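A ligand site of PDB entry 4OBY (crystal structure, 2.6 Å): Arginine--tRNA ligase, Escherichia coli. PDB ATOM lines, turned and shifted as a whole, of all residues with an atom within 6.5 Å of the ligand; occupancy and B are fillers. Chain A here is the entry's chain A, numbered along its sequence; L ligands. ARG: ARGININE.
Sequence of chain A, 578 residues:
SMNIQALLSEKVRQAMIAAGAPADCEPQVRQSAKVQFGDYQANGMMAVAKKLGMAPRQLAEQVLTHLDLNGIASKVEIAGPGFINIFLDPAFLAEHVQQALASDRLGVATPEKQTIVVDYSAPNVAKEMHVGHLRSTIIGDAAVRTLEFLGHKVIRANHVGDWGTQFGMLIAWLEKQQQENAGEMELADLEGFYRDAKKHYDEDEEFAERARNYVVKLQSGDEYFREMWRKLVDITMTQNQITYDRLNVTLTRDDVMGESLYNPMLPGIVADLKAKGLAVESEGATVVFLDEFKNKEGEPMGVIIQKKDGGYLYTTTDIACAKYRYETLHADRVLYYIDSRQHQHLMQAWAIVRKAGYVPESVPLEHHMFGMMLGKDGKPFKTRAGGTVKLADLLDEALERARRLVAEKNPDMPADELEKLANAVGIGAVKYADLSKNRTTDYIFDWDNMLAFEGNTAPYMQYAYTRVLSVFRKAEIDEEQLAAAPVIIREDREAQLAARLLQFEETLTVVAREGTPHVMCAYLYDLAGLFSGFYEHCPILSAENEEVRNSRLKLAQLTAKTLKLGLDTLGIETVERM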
ATOM      1  N   ASP A 119      14.848  18.271  -4.250  1.00  0.00           N
ATOM      2  CA  ASP A 119      14.740  18.291  -2.804  1.00  0.00           C
ATOM      3  C   ASP A 119      13.667  19.266  -2.401  1.00  0.00           C
ATOM      4  O   ASP A 119      13.932  20.469  -2.378  1.00  0.00           O
ATOM      5  CB  ASP A 119      16.099  18.684  -2.201  1.00  0.00           C
ATOM      6  CG  ASP A 119      16.182  18.481  -0.697  1.00  0.00           C
ATOM      7  OD1 ASP A 119      15.198  18.715   0.026  1.00  0.00           O
ATOM      8  OD2 ASP A 119      17.270  18.096  -0.223  1.00  0.00           O
ATOM      9  N   SER A 121       9.691  20.108  -0.012  1.00  0.00           N
ATOM     10  CA  SER A 121       8.752  19.865   1.089  1.00  0.00           C
ATOM     11  C   SER A 121       9.535  19.769   2.366  1.00  0.00           C
ATOM     12  O   SER A 121       9.637  20.735   3.111  1.00  0.00           O
ATOM     13  CB  SER A 121       7.914  18.613   0.887  1.00  0.00           C
ATOM     14  OG  SER A 121       6.898  18.509   1.875  1.00  0.00           O
ATOM     15  N   ALA A 122      10.080  18.583   2.604  1.00  0.00           N
ATOM     16  CA  ALA A 122      11.030  18.312   3.696  1.00  0.00           C
ATOM     17  C   ALA A 122      10.583  18.746   5.105  1.00  0.00           C
ATOM     18  O   ALA A 122      11.311  19.451   5.793  1.00  0.00           O
ATOM     19  CB  ALA A 122      12.382  18.955   3.360  1.00  0.00           C
ATOM     20  N   PRO A 123       9.393  18.298   5.547  1.00  0.00           N
ATOM     21  CA  PRO A 123       8.960  18.576   6.924  1.00  0.00           C
ATOM     22  C   PRO A 123       9.766  17.838   7.987  1.00  0.00           C
ATOM     23  O   PRO A 123      10.654  17.050   7.659  1.00  0.00           O
ATOM     24  CB  PRO A 123       7.518  18.070   6.928  1.00  0.00           C
ATOM     25  CG  PRO A 123       7.485  17.037   5.889  1.00  0.00           C
ATOM     26  CD  PRO A 123       8.368  17.538   4.807  1.00  0.00           C
ATOM     27  N   ASN A 124       9.438  18.067   9.258  1.00  0.00           N
ATOM     28  CA  ASN A 124      10.108  17.418  10.377  1.00  0.00           C
ATOM     29  C   ASN A 124       9.166  16.519  11.178  1.00  0.00           C
ATOM     30  O   ASN A 124       8.004  16.861  11.356  1.00  0.00           O
ATOM     31  CB  ASN A 124      10.719  18.460  11.306  1.00  0.00           C
ATOM     32  CG  ASN A 124      11.764  19.316  10.610  1.00  0.00           C
ATOM     33  OD1 ASN A 124      12.557  18.832   9.808  1.00  0.00           O
ATOM     34  ND2 ASN A 124      11.762  20.594  10.923  1.00  0.00           N
ATOM     35  N   HIS A 130       4.640  23.238   8.521  1.00  0.00           N
ATOM     36  CA  HIS A 130       4.320  24.660   8.520  1.00  0.00           C
ATOM     37  C   HIS A 130       4.426  25.319   7.122  1.00  0.00           C
ATOM     38  O   HIS A 130       4.752  24.656   6.150  1.00  0.00           O
ATOM     39  CB  HIS A 130       5.208  25.406   9.534  1.00  0.00           C
ATOM     40  CG  HIS A 130       6.670  25.362   9.220  1.00  0.00           C
ATOM     41  ND1 HIS A 130       7.189  25.791   8.013  1.00  0.00           N
ATOM     42  CD2 HIS A 130       7.734  24.976   9.958  1.00  0.00           C
ATOM     43  CE1 HIS A 130       8.501  25.643   8.020  1.00  0.00           C
ATOM     44  NE2 HIS A 130       8.856  25.150   9.197  1.00  0.00           N
ATOM     45  N   HIS A 133       7.323  24.669   4.542  1.00  0.00           N
ATOM     46  CA  HIS A 133       7.190  23.393   3.889  1.00  0.00           C
ATOM     47  C   HIS A 133       6.054  23.454   2.906  1.00  0.00           C
ATOM     48  O   HIS A 133       6.096  22.806   1.857  1.00  0.00           O
ATOM     49  CB  HIS A 133       6.926  22.285   4.895  1.00  0.00           C
ATOM     50  CG  HIS A 133       7.899  22.239   6.022  1.00  0.00           C
ATOM     51  ND1 HIS A 133       7.510  22.252   7.341  1.00  0.00           N
ATOM     52  CD2 HIS A 133       9.254  22.173   6.031  1.00  0.00           C
ATOM     53  CE1 HIS A 133       8.580  22.192   8.118  1.00  0.00           C
ATOM     54  NE2 HIS A 133       9.652  22.131   7.337  1.00  0.00           N
ATOM     55  N   HIS A 159      13.280  15.362   1.848  1.00  0.00           N
ATOM     56  CA  HIS A 159      14.378  15.340   2.821  1.00  0.00           C
ATOM     57  C   HIS A 159      13.890  15.554   4.247  1.00  0.00           C
ATOM     58  O   HIS A 159      14.208  16.548   4.892  1.00  0.00           O
ATOM     59  CB  HIS A 159      15.396  16.409   2.436  1.00  0.00           C
ATOM     60  CG  HIS A 159      16.750  16.209   3.037  1.00  0.00           C
ATOM     61  ND1 HIS A 159      17.664  15.308   2.542  1.00  0.00           N
ATOM     62  CD2 HIS A 159      17.354  16.833   4.082  1.00  0.00           C
ATOM     63  CE1 HIS A 159      18.772  15.379   3.247  1.00  0.00           C
ATOM     64  NE2 HIS A 159      18.607  16.288   4.200  1.00  0.00           N
ATOM     65  N   VAL A 160      13.130  14.601   4.744  1.00  0.00           N
ATOM     66  CA  VAL A 160      12.489  14.782   6.034  1.00  0.00           C
ATOM     67  C   VAL A 160      13.487  14.823   7.213  1.00  0.00           C
ATOM     68  O   VAL A 160      14.384  13.997   7.309  1.00  0.00           O
ATOM     69  CB  VAL A 160      11.463  13.662   6.262  1.00  0.00           C
ATOM     70  CG1 VAL A 160      10.848  13.770   7.636  1.00  0.00           C
ATOM     71  CG2 VAL A 160      10.405  13.719   5.193  1.00  0.00           C
ATOM     72  N   GLY A 161      13.297  15.806   8.104  1.00  0.00           N
ATOM     73  CA  GLY A 161      14.018  15.890   9.364  1.00  0.00           C
ATOM     74  C   GLY A 161      13.568  14.805  10.335  1.00  0.00           C
ATOM     75  O   GLY A 161      12.742  15.041  11.226  1.00  0.00           O
ATOM     76  N   GLU A 259      16.863  12.560   6.664  1.00  0.00           N
ATOM     77  CA  GLU A 259      18.238  12.729   7.099  1.00  0.00           C
ATOM     78  C   GLU A 259      18.821  11.402   7.574  1.00  0.00           C
ATOM     79  O   GLU A 259      20.001  11.109   7.341  1.00  0.00           O
ATOM     80  CB  GLU A 259      18.330  13.744   8.224  1.00  0.00           C
ATOM     81  CG  GLU A 259      18.102  15.181   7.832  1.00  0.00           C
ATOM     82  CD  GLU A 259      18.134  16.046   9.053  1.00  0.00           C
ATOM     83  OE1 GLU A 259      17.249  15.851   9.935  1.00  0.00           O
ATOM     84  OE2 GLU A 259      19.048  16.883   9.153  1.00  0.00           O
ATOM     85  N   TYR A 314      23.314  19.131  10.700  1.00  0.00           N
ATOM     86  CA  TYR A 314      22.517  19.428   9.522  1.00  0.00           C
ATOM     87  C   TYR A 314      23.459  19.636   8.323  1.00  0.00           C
ATOM     88  O   TYR A 314      23.220  19.167   7.226  1.00  0.00           O
ATOM     89  CB  TYR A 314      21.649  20.632   9.843  1.00  0.00           C
ATOM     90  CG  TYR A 314      20.625  21.026   8.820  1.00  0.00           C
ATOM     91  CD1 TYR A 314      19.811  20.074   8.235  1.00  0.00           C
ATOM     92  CD2 TYR A 314      20.445  22.354   8.481  1.00  0.00           C
ATOM     93  CE1 TYR A 314      18.869  20.428   7.308  1.00  0.00           C
ATOM     94  CE2 TYR A 314      19.495  22.727   7.554  1.00  0.00           C
ATOM     95  CZ  TYR A 314      18.717  21.768   6.976  1.00  0.00           C
ATOM     96  OH  TYR A 314      17.780  22.135   6.048  1.00  0.00           O
ATOM     97  N   THR A 317      24.783  16.125   7.152  1.00  0.00           N
ATOM     98  CA  THR A 317      23.736  15.433   6.450  1.00  0.00           C
ATOM     99  C   THR A 317      23.453  16.099   5.085  1.00  0.00           C
ATOM    100  O   THR A 317      23.047  15.417   4.156  1.00  0.00           O
ATOM    101  CB  THR A 317      22.465  15.364   7.317  1.00  0.00           C
ATOM    102  OG1 THR A 317      21.584  14.376   6.780  1.00  0.00           O
ATOM    103  CG2 THR A 317      21.730  16.666   7.339  1.00  0.00           C
ATOM    104  N   ASP A 318      23.693  17.406   4.952  1.00  0.00           N
ATOM    105  CA  ASP A 318      23.528  18.034   3.630  1.00  0.00           C
ATOM    106  C   ASP A 318      24.752  17.751   2.759  1.00  0.00           C
ATOM    107  O   ASP A 318      24.677  17.794   1.536  1.00  0.00           O
ATOM    108  CB  ASP A 318      23.300  19.550   3.726  1.00  0.00           C
ATOM    109  CG  ASP A 318      21.810  19.919   3.760  1.00  0.00           C
ATOM    110  OD1 ASP A 318      21.025  19.381   2.956  1.00  0.00           O
ATOM    111  OD2 ASP A 318      21.432  20.762   4.615  1.00  0.00           O
ATOM    112  N   CYS A 321      24.071  13.910   1.619  1.00  0.00           N
ATOM    113  CA  CYS A 321      22.962  14.005   0.712  1.00  0.00           C
ATOM    114  C   CYS A 321      23.391  14.479  -0.671  1.00  0.00           C
ATOM    115  O   CYS A 321      22.960  13.947  -1.677  1.00  0.00           O
ATOM    116  CB  CYS A 321      21.914  14.911   1.379  1.00  0.00           C
ATOM    117  SG  CYS A 321      21.035  16.020   0.389  1.00  0.00           S
ATOM    118  N   ARG A 325      23.532  11.819  -3.866  1.00  0.00           N
ATOM    119  CA  ARG A 325      22.707  12.084  -5.019  1.00  0.00           C
ATOM    120  C   ARG A 325      23.511  12.010  -6.320  1.00  0.00           C
ATOM    121  O   ARG A 325      22.980  11.661  -7.389  1.00  0.00           O
ATOM    122  CB  ARG A 325      22.037  13.447  -4.876  1.00  0.00           C
ATOM    123  CG  ARG A 325      20.892  13.420  -3.901  1.00  0.00           C
ATOM    124  CD  ARG A 325      20.418  14.814  -3.535  1.00  0.00           C
ATOM    125  NE  ARG A 325      19.396  14.709  -2.496  1.00  0.00           N
ATOM    126  CZ  ARG A 325      18.847  15.757  -1.891  1.00  0.00           C
ATOM    127  NH1 ARG A 325      19.249  16.983  -2.203  1.00  0.00           N
ATOM    128  NH2 ARG A 325      17.928  15.581  -0.957  1.00  0.00           N
ATOM    129  N   TYR A 336      17.198  22.464  -4.843  1.00  0.00           N
ATOM    130  CA  TYR A 336      16.828  22.563  -3.430  1.00  0.00           C
ATOM    131  C   TYR A 336      15.833  23.703  -3.215  1.00  0.00           C
ATOM    132  O   TYR A 336      16.184  24.895  -3.229  1.00  0.00           O
ATOM    133  CB  TYR A 336      18.054  22.792  -2.564  1.00  0.00           C
ATOM    134  CG  TYR A 336      19.052  21.681  -2.560  1.00  0.00           C
ATOM    135  CD1 TYR A 336      19.928  21.513  -3.640  1.00  0.00           C
ATOM    136  CD2 TYR A 336      19.157  20.807  -1.479  1.00  0.00           C
ATOM    137  CE1 TYR A 336      20.883  20.481  -3.637  1.00  0.00           C
ATOM    138  CE2 TYR A 336      20.088  19.788  -1.454  1.00  0.00           C
ATOM    139  CZ  TYR A 336      20.951  19.625  -2.534  1.00  0.00           C
ATOM    140  OH  TYR A 336      21.869  18.612  -2.519  1.00  0.00           O
ATOM    141  N   TYR A 337      14.593  23.316  -3.005  1.00  0.00           N
ATOM    142  CA  TYR A 337      13.552  24.268  -2.693  1.00  0.00           C
ATOM    143  C   TYR A 337      13.466  24.438  -1.198  1.00  0.00           C
ATOM    144  O   TYR A 337      12.649  23.790  -0.535  1.00  0.00           O
ATOM    145  CB  TYR A 337      12.223  23.801  -3.285  1.00  0.00           C
ATOM    146  CG  TYR A 337      12.233  23.988  -4.785  1.00  0.00           C
ATOM    147  CD1 TYR A 337      11.977  25.226  -5.344  1.00  0.00           C
ATOM    148  CD2 TYR A 337      12.548  22.948  -5.632  1.00  0.00           C
ATOM    149  CE1 TYR A 337      11.995  25.410  -6.684  1.00  0.00           C
ATOM    150  CE2 TYR A 337      12.572  23.134  -7.004  1.00  0.00           C
ATOM    151  CZ  TYR A 337      12.302  24.367  -7.520  1.00  0.00           C
ATOM    152  OH  TYR A 337      12.314  24.592  -8.863  1.00  0.00           O
ATOM    153  N   ILE A 338      14.347  25.286  -0.673  1.00  0.00           N
ATOM    154  CA  ILE A 338      14.426  25.594   0.749  1.00  0.00           C
ATOM    155  C   ILE A 338      14.299  27.111   0.987  1.00  0.00           C
ATOM    156  O   ILE A 338      14.893  27.894   0.244  1.00  0.00           O
ATOM    157  CB  ILE A 338      15.776  25.147   1.416  1.00  0.00           C
ATOM    158  CG1 ILE A 338      16.275  23.750   0.978  1.00  0.00           C
ATOM    159  CG2 ILE A 338      15.721  25.351   2.926  1.00  0.00           C
ATOM    160  CD1 ILE A 338      15.243  22.664   0.973  1.00  0.00           C
ATOM    161  N   GLN A 342      17.939  29.718   4.988  1.00  0.00           N
ATOM    162  CA  GLN A 342      18.957  28.669   5.006  1.00  0.00           C
ATOM    163  C   GLN A 342      20.030  28.826   3.930  1.00  0.00           C
ATOM    164  O   GLN A 342      20.828  27.921   3.737  1.00  0.00           O
ATOM    165  CB  GLN A 342      18.301  27.297   4.847  1.00  0.00           C
ATOM    166  CG  GLN A 342      17.149  27.051   5.765  1.00  0.00           C
ATOM    167  CD  GLN A 342      17.006  25.573   6.071  1.00  0.00           C
ATOM    168  OE1 GLN A 342      17.919  24.797   5.810  1.00  0.00           O
ATOM    169  NE2 GLN A 342      15.862  25.179   6.635  1.00  0.00           N
ATOM    170  N   HIS A 345      23.675  28.379   4.842  1.00  0.00           N
ATOM    171  CA  HIS A 345      23.864  27.003   5.294  1.00  0.00           C
ATOM    172  C   HIS A 345      24.189  26.140   4.093  1.00  0.00           C
ATOM    173  O   HIS A 345      25.215  25.469   4.058  1.00  0.00           O
ATOM    174  CB  HIS A 345      22.645  26.456   6.006  1.00  0.00           C
ATOM    175  CG  HIS A 345      22.637  24.971   6.129  1.00  0.00           C
ATOM    176  ND1 HIS A 345      23.524  24.280   6.921  1.00  0.00           N
ATOM    177  CD2 HIS A 345      21.838  24.037   5.552  1.00  0.00           C
ATOM    178  CE1 HIS A 345      23.277  22.986   6.832  1.00  0.00           C
ATOM    179  NE2 HIS A 345      22.262  22.808   6.005  1.00  0.00           N
ATOM    180  N   LEU A 346      23.304  26.192   3.100  1.00  0.00           N
ATOM    181  CA  LEU A 346      23.513  25.476   1.860  1.00  0.00           C
ATOM    182  C   LEU A 346      24.803  25.847   1.163  1.00  0.00           C
ATOM    183  O   LEU A 346      25.450  25.000   0.587  1.00  0.00           O
ATOM    184  CB  LEU A 346      22.368  25.706   0.908  1.00  0.00           C
ATOM    185  CG  LEU A 346      21.037  25.161   1.387  1.00  0.00           C
ATOM    186  CD1 LEU A 346      19.904  25.709   0.505  1.00  0.00           C
ATOM    187  CD2 LEU A 346      21.134  23.639   1.363  1.00  0.00           C
HETATM  188  N   ARG L   1      13.387  19.621   7.114  1.00  0.00           N
HETATM  189  CA  ARG L   1      14.203  20.818   7.220  1.00  0.00           C
HETATM  190  C   ARG L   1      13.420  21.938   7.921  1.00  0.00           C
HETATM  191  O   ARG L   1      13.910  23.072   8.070  1.00  0.00           O
HETATM  192  CB  ARG L   1      14.689  21.283   5.833  1.00  0.00           C
HETATM  193  CG  ARG L   1      15.587  20.272   5.085  1.00  0.00           C
HETATM  194  CD  ARG L   1      15.840  20.805   3.692  1.00  0.00           C
HETATM  195  NE  ARG L   1      16.667  20.009   2.776  1.00  0.00           N
HETATM  196  CZ  ARG L   1      18.001  19.978   2.825  1.00  0.00           C
HETATM  197  NH1 ARG L   1      18.666  20.624   3.804  1.00  0.00           N
HETATM  198  NH2 ARG L   1      18.681  19.286   1.925  1.00  0.00           N
HETATM  199  OXT ARG L   1      12.274  21.734   8.354  1.00  0.00           O
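N of the ligand sits at hydrogen-bond distance from O of Ala 122, at 2.5 Å.
The side-chain carboxylate (OD1) of Asp 318 is in salt-bridge range of a nitrogen (NH2) of the ligand.
OD2 of Asp 119 lies within salt-bridge range of NH2 of the ligand (2.8 Å).
An oxygen (OXT) of the ligand lies within hydrogen-bond range of a ring nitrogen (NE2) of His 133.
NH1 of the ligand lies within hydrogen-bond range of OH of Tyr 314, at 2.8 Å.
ND2 of Asn 124 is in hydrogen-bond range of OXT of the ligand (2.9 Å).
NE2 of Gln 342 is in hydrogen-bond range of O of the ligand (3.2 Å).
The side-chain carboxylate (OD2) of Asp 318 lies within hydrogen-bond range of a ring nitrogen (NE2) of His 345 (2.6 Å).
The guanidinium group (NH2) of Arg 325 is in salt-bridge range of the side-chain carboxylate (OD2) of Asp 119 (2.7 Å).
N of Tyr 337 lies within hydrogen-bond range of O of Asp 119 (3.0 Å).
ND1 of His 133 lies within hydrogen-bond range of N of His 130 (3.3 Å).
The side-chain hydroxyl of Tyr 314 lies within hydrogen-bond range of the side-chain amide oxygen of Gln 342 (2.7 Å).
NH1 of Arg 325 lies close to OH of Tyr 336, at 3.1 Å.
O of Pro 123 sits at hydrogen-bond distance from N of Gly 161.
Merely in contact with the ligand: Ile 338 (3.3 Å), His 159 (3.4 Å), Tyr 336 (3.7 Å), Pro 123 (3.8 Å) and Gly 161 (3.9 Å).
Hydrophobic or aromatic side chains that line the ligand: Ala 122, His 133, His 159, Tyr 314, Tyr 336 and Ile 338.
Of the 22 residues printed, 12 come within 4 Å of the ligand.
The nearest printed residue that does not touch the ligand is Cys 321 (4.3 Å).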
